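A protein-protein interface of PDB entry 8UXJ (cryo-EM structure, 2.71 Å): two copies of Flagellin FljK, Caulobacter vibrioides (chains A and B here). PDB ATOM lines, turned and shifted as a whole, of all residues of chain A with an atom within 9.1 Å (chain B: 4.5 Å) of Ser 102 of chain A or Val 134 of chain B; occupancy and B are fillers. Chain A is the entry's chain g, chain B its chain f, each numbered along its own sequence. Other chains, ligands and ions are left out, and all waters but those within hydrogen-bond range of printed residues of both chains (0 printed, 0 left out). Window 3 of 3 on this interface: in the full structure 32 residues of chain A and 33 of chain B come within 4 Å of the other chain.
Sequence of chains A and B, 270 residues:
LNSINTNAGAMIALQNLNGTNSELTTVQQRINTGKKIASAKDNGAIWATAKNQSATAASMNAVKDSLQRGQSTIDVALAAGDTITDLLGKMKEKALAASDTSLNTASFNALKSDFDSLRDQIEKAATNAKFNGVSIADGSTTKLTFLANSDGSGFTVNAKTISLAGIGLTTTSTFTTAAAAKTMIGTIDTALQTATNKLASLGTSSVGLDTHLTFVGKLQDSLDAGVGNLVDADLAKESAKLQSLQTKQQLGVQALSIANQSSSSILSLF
The side-chain hydroxyl (OG) of Ser 107 of chain A lies within hydrogen-bond range of the backbone carbonyl oxygen (O) of Asn 104 of chain A (3.1 Å).
Hydrophobic or aromatic side chains of chain B that line the printed part of chain A: Val 134 and Phe 146.
Of the 13 printed residues of chain A, 5 touch a printed residue of chain B.
Among the printed residues, Asp or Glu carboxylates within 4 Å of a Lys or Arg side-chain nitrogen of the other chain: Asp 100 of chain A with Arg 69 of chain B (3.9 Å).
No position is printed for both chains.
Of the 9 pairs that touch across the chains among the printed residues, none has its exchanged pair printed and touching as well.
Among the printed residues, merely in contact across the chains: Asp 100 of chain A with Phe 146 of chain B (3.4 Å), Ser 102 of chain A with Val 134 of chain B (3.4 Å), Ser 102 of chain A with Phe 146 of chain B (3.8 Å) and Asn 104 of chain A with Asn 132 of chain B (3.8 Å).
Of the printed residues of chain B, Asp 100 of chain A touches Arg 69 (3.9 Å), Thr 145 (3.1 Å) and Phe 146 (3.4 Å).
Ser 102 of chain A touches just these residues of chain B: Arg 69 (3.3 Å), Val 134 (3.4 Å) and Phe 146 (3.8 Å).
Of the printed residues of chain B, Leu 103 of chain A touches Arg 69.
Printed residues of chain B within 4 Å of Asn 104 of chain A: Asn 132.
Printed residues of chain A within 4 Å of Arg 69 of chain B: Asp 100 (3.9 Å), Ser 102 (3.3 Å) and Leu 103 (3.1 Å).
No residue of chain A comes within 4 Å of Gly 133 of chain B.
No residue of chain A comes within 4 Å of Ser 135 of chain B.
Of the printed residues of chain A, Phe 146 of chain B touches Asp 100 and Ser 102.
The side-chain carboxylate (OD2) of Asp 100 of chain A sits close to the backbone carbonyl oxygen (O) of Thr 145 of chain B (3.1 Å).
The backbone NH of Leu 103 of chain A sits close to the guanidinium group of Arg 69 of chain B, 3.1 Å away.
The backbone carbonyl oxygen (O) of Thr 145 of chain B lies within hydrogen-bond range of the side-chain hydroxyl (OG1) of Thr 101 of chain A (3.4 Å).
The guanidinium group (NH1) of Arg 69 of chain B sits at hydrogen-bond distance from the side-chain hydroxyl (OG) of Ser 102 of chain A (3.3 Å).
The guanidinium group of Arg 69 of chain B lies within salt-bridge range of the side-chain carboxylate of Asp 100 of chain A (3.9 Å).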
ATOM      1  N   ALA A  97     -17.617  27.538   9.679  1.00  0.00           N
ATOM      2  CA  ALA A  97     -17.032  26.209   9.839  1.00  0.00           C
ATOM      3  C   ALA A  97     -18.074  25.217  10.334  1.00  0.00           C
ATOM      4  O   ALA A  97     -18.101  24.059   9.902  1.00  0.00           O
ATOM      5  CB  ALA A  97     -15.840  26.262  10.794  1.00  0.00           C
ATOM      6  N   ALA A  98     -18.951  25.661  11.234  1.00  0.00           N
ATOM      7  CA  ALA A  98     -20.025  24.804  11.709  1.00  0.00           C
ATOM      8  C   ALA A  98     -20.914  24.330  10.565  1.00  0.00           C
ATOM      9  O   ALA A  98     -21.414  23.198  10.587  1.00  0.00           O
ATOM     10  CB  ALA A  98     -20.851  25.570  12.733  1.00  0.00           C
ATOM     11  N   SER A  99     -21.125  25.185   9.559  1.00  0.00           N
ATOM     12  CA  SER A  99     -22.121  24.895   8.528  1.00  0.00           C
ATOM     13  C   SER A  99     -21.830  23.597   7.783  1.00  0.00           C
ATOM     14  O   SER A  99     -22.757  22.941   7.298  1.00  0.00           O
ATOM     15  CB  SER A  99     -22.217  26.067   7.557  1.00  0.00           C
ATOM     16  OG  SER A  99     -22.691  27.209   8.239  1.00  0.00           O
ATOM     17  N   ASP A 100     -20.562  23.218   7.662  1.00  0.00           N
ATOM     18  CA  ASP A 100     -20.226  21.993   6.946  1.00  0.00           C
ATOM     19  C   ASP A 100     -20.800  20.800   7.702  1.00  0.00           C
ATOM     20  O   ASP A 100     -20.981  20.848   8.920  1.00  0.00           O
ATOM     21  CB  ASP A 100     -18.704  21.877   6.795  1.00  0.00           C
ATOM     22  CG  ASP A 100     -18.255  20.591   6.100  1.00  0.00           C
ATOM     23  OD1 ASP A 100     -17.275  20.680   5.331  1.00  0.00           O
ATOM     24  OD2 ASP A 100     -18.853  19.512   6.284  1.00  0.00           O
ATOM     25  N   THR A 101     -21.161  19.750   6.961  1.00  0.00           N
ATOM     26  CA  THR A 101     -21.692  18.546   7.592  1.00  0.00           C
ATOM     27  C   THR A 101     -20.584  17.670   8.170  1.00  0.00           C
ATOM     28  O   THR A 101     -20.792  16.972   9.168  1.00  0.00           O
ATOM     29  CB  THR A 101     -22.518  17.750   6.584  1.00  0.00           C
ATOM     30  OG1 THR A 101     -21.681  17.346   5.492  1.00  0.00           O
ATOM     31  CG2 THR A 101     -23.657  18.599   6.045  1.00  0.00           C
ATOM     32  N   SER A 102     -19.403  17.688   7.546  1.00  0.00           N
ATOM     33  CA  SER A 102     -18.443  16.596   7.713  1.00  0.00           C
ATOM     34  C   SER A 102     -17.908  16.489   9.141  1.00  0.00           C
ATOM     35  O   SER A 102     -17.603  15.386   9.610  1.00  0.00           O
ATOM     36  CB  SER A 102     -17.293  16.765   6.719  1.00  0.00           C
ATOM     37  OG  SER A 102     -16.331  15.739   6.874  1.00  0.00           O
ATOM     38  N   LEU A 103     -17.759  17.617   9.837  1.00  0.00           N
ATOM     39  CA  LEU A 103     -17.085  17.602  11.132  1.00  0.00           C
ATOM     40  C   LEU A 103     -17.881  16.790  12.146  1.00  0.00           C
ATOM     41  O   LEU A 103     -19.115  16.788  12.139  1.00  0.00           O
ATOM     42  CB  LEU A 103     -16.860  19.026  11.656  1.00  0.00           C
ATOM     43  CG  LEU A 103     -18.042  19.844  12.185  1.00  0.00           C
ATOM     44  CD1 LEU A 103     -17.561  21.046  12.977  1.00  0.00           C
ATOM     45  CD2 LEU A 103     -18.947  20.284  11.063  1.00  0.00           C
ATOM     46  N   ASN A 104     -17.157  16.081  13.007  1.00  0.00           N
ATOM     47  CA  ASN A 104     -17.761  15.254  14.035  1.00  0.00           C
ATOM     48  C   ASN A 104     -18.305  16.142  15.158  1.00  0.00           C
ATOM     49  O   ASN A 104     -17.988  17.330  15.255  1.00  0.00           O
ATOM     50  CB  ASN A 104     -16.732  14.247  14.550  1.00  0.00           C
ATOM     51  CG  ASN A 104     -17.330  13.207  15.468  1.00  0.00           C
ATOM     52  OD1 ASN A 104     -18.523  13.232  15.764  1.00  0.00           O
ATOM     53  ND2 ASN A 104     -16.501  12.273  15.914  1.00  0.00           N
ATOM     54  N   THR A 105     -19.139  15.543  16.014  1.00  0.00           N
ATOM     55  CA  THR A 105     -19.925  16.317  16.974  1.00  0.00           C
ATOM     56  C   THR A 105     -19.053  17.077  17.970  1.00  0.00           C
ATOM     57  O   THR A 105     -19.460  18.130  18.476  1.00  0.00           O
ATOM     58  CB  THR A 105     -20.903  15.399  17.709  1.00  0.00           C
ATOM     59  OG1 THR A 105     -21.781  16.184  18.525  1.00  0.00           O
ATOM     60  CG2 THR A 105     -20.166  14.384  18.572  1.00  0.00           C
ATOM     61  N   ALA A 106     -17.865  16.555  18.288  1.00  0.00           N
ATOM     62  CA  ALA A 106     -17.035  17.195  19.307  1.00  0.00           C
ATOM     63  C   ALA A 106     -16.625  18.604  18.888  1.00  0.00           C
ATOM     64  O   ALA A 106     -16.840  19.574  19.628  1.00  0.00           O
ATOM     65  CB  ALA A 106     -15.799  16.341  19.582  1.00  0.00           C
ATOM     66  N   SER A 107     -16.060  18.739  17.687  1.00  0.00           N
ATOM     67  CA  SER A 107     -15.665  20.052  17.185  1.00  0.00           C
ATOM     68  C   SER A 107     -16.879  20.944  16.966  1.00  0.00           C
ATOM     69  O   SER A 107     -16.802  22.168  17.127  1.00  0.00           O
ATOM     70  CB  SER A 107     -14.866  19.884  15.895  1.00  0.00           C
ATOM     71  OG  SER A 107     -15.679  19.353  14.865  1.00  0.00           O
ATOM     72  N   PHE A 108     -18.007  20.347  16.577  1.00  0.00           N
ATOM     73  CA  PHE A 108     -19.245  21.098  16.409  1.00  0.00           C
ATOM     74  C   PHE A 108     -19.655  21.767  17.720  1.00  0.00           C
ATOM     75  O   PHE A 108     -19.978  22.963  17.753  1.00  0.00           O
ATOM     76  CB  PHE A 108     -20.316  20.127  15.897  1.00  0.00           C
ATOM     77  CG  PHE A 108     -21.661  20.740  15.623  1.00  0.00           C
ATOM     78  CD1 PHE A 108     -22.488  21.169  16.649  1.00  0.00           C
ATOM     79  CD2 PHE A 108     -22.111  20.846  14.320  1.00  0.00           C
ATOM     80  CE1 PHE A 108     -23.721  21.710  16.373  1.00  0.00           C
ATOM     81  CE2 PHE A 108     -23.343  21.388  14.042  1.00  0.00           C
ATOM     82  CZ  PHE A 108     -24.149  21.815  15.069  1.00  0.00           C
ATOM     83  N   ALA A 178     -25.746  21.172  11.005  1.00  0.00           N
ATOM     84  CA  ALA A 178     -25.068  21.845   9.902  1.00  0.00           C
ATOM     85  C   ALA A 178     -26.035  22.720   9.110  1.00  0.00           C
ATOM     86  O   ALA A 178     -25.690  23.838   8.700  1.00  0.00           O
ATOM     87  CB  ALA A 178     -24.406  20.815   8.989  1.00  0.00           C
ATOM     88  N   ARG B  69      -9.824  18.919   4.634  1.00  0.00           N
ATOM     89  CA  ARG B  69     -10.462  17.719   5.165  1.00  0.00           C
ATOM     90  C   ARG B  69     -11.037  16.865   4.045  1.00  0.00           C
ATOM     91  O   ARG B  69     -10.929  15.631   4.068  1.00  0.00           O
ATOM     92  CB  ARG B  69     -11.544  18.120   6.167  1.00  0.00           C
ATOM     93  CG  ARG B  69     -10.998  18.400   7.563  1.00  0.00           C
ATOM     94  CD  ARG B  69     -12.069  18.301   8.639  1.00  0.00           C
ATOM     95  NE  ARG B  69     -13.019  19.404   8.566  1.00  0.00           N
ATOM     96  CZ  ARG B  69     -14.337  19.265   8.569  1.00  0.00           C
ATOM     97  NH1 ARG B  69     -14.905  18.073   8.639  1.00  0.00           N
ATOM     98  NH2 ARG B  69     -15.103  20.349   8.505  1.00  0.00           N
ATOM     99  N   LYS B 130     -11.587   5.242   6.824  1.00  0.00           N
ATOM    100  CA  LYS B 130     -12.313   6.419   7.288  1.00  0.00           C
ATOM    101  C   LYS B 130     -11.309   7.471   7.736  1.00  0.00           C
ATOM    102  O   LYS B 130     -10.143   7.170   8.000  1.00  0.00           O
ATOM    103  CB  LYS B 130     -13.268   6.089   8.444  1.00  0.00           C
ATOM    104  CG  LYS B 130     -14.403   5.138   8.107  1.00  0.00           C
ATOM    105  CD  LYS B 130     -15.323   4.934   9.292  1.00  0.00           C
ATOM    106  CE  LYS B 130     -14.641   4.122  10.376  1.00  0.00           C
ATOM    107  NZ  LYS B 130     -14.373   2.733   9.921  1.00  0.00           N
ATOM    108  N   PHE B 131     -11.781   8.714   7.818  1.00  0.00           N
ATOM    109  CA  PHE B 131     -10.981   9.817   8.340  1.00  0.00           C
ATOM    110  C   PHE B 131     -11.876  10.691   9.205  1.00  0.00           C
ATOM    111  O   PHE B 131     -12.917  11.162   8.739  1.00  0.00           O
ATOM    112  CB  PHE B 131     -10.350  10.637   7.208  1.00  0.00           C
ATOM    113  CG  PHE B 131      -9.698  11.912   7.670  1.00  0.00           C
ATOM    114  CD1 PHE B 131      -8.383  11.914   8.096  1.00  0.00           C
ATOM    115  CD2 PHE B 131     -10.392  13.110   7.661  1.00  0.00           C
ATOM    116  CE1 PHE B 131      -7.779  13.079   8.520  1.00  0.00           C
ATOM    117  CE2 PHE B 131      -9.790  14.277   8.083  1.00  0.00           C
ATOM    118  CZ  PHE B 131      -8.483  14.261   8.512  1.00  0.00           C
ATOM    119  N   ASN B 132     -11.460  10.906  10.455  1.00  0.00           N
ATOM    120  CA  ASN B 132     -12.227  11.679  11.436  1.00  0.00           C
ATOM    121  C   ASN B 132     -13.640  11.108  11.579  1.00  0.00           C
ATOM    122  O   ASN B 132     -14.627  11.839  11.674  1.00  0.00           O
ATOM    123  CB  ASN B 132     -12.259  13.167  11.065  1.00  0.00           C
ATOM    124  CG  ASN B 132     -12.853  14.046  12.162  1.00  0.00           C
ATOM    125  OD1 ASN B 132     -13.275  13.561  13.211  1.00  0.00           O
ATOM    126  ND2 ASN B 132     -12.892  15.350  11.914  1.00  0.00           N
ATOM    127  N   GLY B 133     -13.741   9.781  11.555  1.00  0.00           N
ATOM    128  CA  GLY B 133     -15.012   9.118  11.751  1.00  0.00           C
ATOM    129  C   GLY B 133     -15.978   9.212  10.594  1.00  0.00           C
ATOM    130  O   GLY B 133     -17.142   8.826  10.749  1.00  0.00           O
ATOM    131  N   VAL B 134     -15.539   9.706   9.438  1.00  0.00           N
ATOM    132  CA  VAL B 134     -16.401   9.897   8.279  1.00  0.00           C
ATOM    133  C   VAL B 134     -15.711   9.300   7.061  1.00  0.00           C
ATOM    134  O   VAL B 134     -14.498   9.457   6.885  1.00  0.00           O
ATOM    135  CB  VAL B 134     -16.721  11.390   8.053  1.00  0.00           C
ATOM    136  CG1 VAL B 134     -17.530  11.581   6.787  1.00  0.00           C
ATOM    137  CG2 VAL B 134     -17.465  11.964   9.247  1.00  0.00           C
ATOM    138  N   SER B 135     -16.483   8.613   6.222  1.00  0.00           N
ATOM    139  CA  SER B 135     -15.958   7.949   5.040  1.00  0.00           C
ATOM    140  C   SER B 135     -16.785   8.319   3.819  1.00  0.00           C
ATOM    141  O   SER B 135     -17.973   8.633   3.922  1.00  0.00           O
ATOM    142  CB  SER B 135     -15.951   6.426   5.204  1.00  0.00           C
ATOM    143  OG  SER B 135     -15.467   5.790   4.035  1.00  0.00           O
ATOM    144  N   LEU B 144     -21.255  14.094   0.788  1.00  0.00           N
ATOM    145  CA  LEU B 144     -20.538  14.857   1.808  1.00  0.00           C
ATOM    146  C   LEU B 144     -20.404  16.296   1.323  1.00  0.00           C
ATOM    147  O   LEU B 144     -19.530  16.607   0.510  1.00  0.00           O
ATOM    148  CB  LEU B 144     -19.172  14.246   2.097  1.00  0.00           C
ATOM    149  CG  LEU B 144     -19.122  13.137   3.146  1.00  0.00           C
ATOM    150  CD1 LEU B 144     -17.702  12.622   3.299  1.00  0.00           C
ATOM    151  CD2 LEU B 144     -19.654  13.637   4.476  1.00  0.00           C
ATOM    152  N   THR B 145     -21.279  17.169   1.812  1.00  0.00           N
ATOM    153  CA  THR B 145     -21.164  18.583   1.502  1.00  0.00           C
ATOM    154  C   THR B 145     -19.929  19.171   2.176  1.00  0.00           C
ATOM    155  O   THR B 145     -19.609  18.859   3.325  1.00  0.00           O
ATOM    156  CB  THR B 145     -22.423  19.328   1.949  1.00  0.00           C
ATOM    157  OG1 THR B 145     -23.561  18.789   1.265  1.00  0.00           O
ATOM    158  CG2 THR B 145     -22.319  20.813   1.638  1.00  0.00           C
ATOM    159  N   PHE B 146     -19.233  20.034   1.444  1.00  0.00           N
ATOM    160  CA  PHE B 146     -18.071  20.740   1.961  1.00  0.00           C
ATOM    161  C   PHE B 146     -18.197  22.221   1.646  1.00  0.00           C
ATOM    162  O   PHE B 146     -18.996  22.635   0.803  1.00  0.00           O
ATOM    163  CB  PHE B 146     -16.737  20.223   1.394  1.00  0.00           C
ATOM    164  CG  PHE B 146     -16.376  18.828   1.826  1.00  0.00           C
ATOM    165  CD1 PHE B 146     -15.810  18.604   3.070  1.00  0.00           C
ATOM    166  CD2 PHE B 146     -16.537  17.752   0.972  1.00  0.00           C
ATOM    167  CE1 PHE B 146     -15.456  17.332   3.469  1.00  0.00           C
ATOM    168  CE2 PHE B 146     -16.181  16.478   1.366  1.00  0.00           C
ATOM    169  CZ  PHE B 146     -15.642  16.269   2.614  1.00  0.00           C
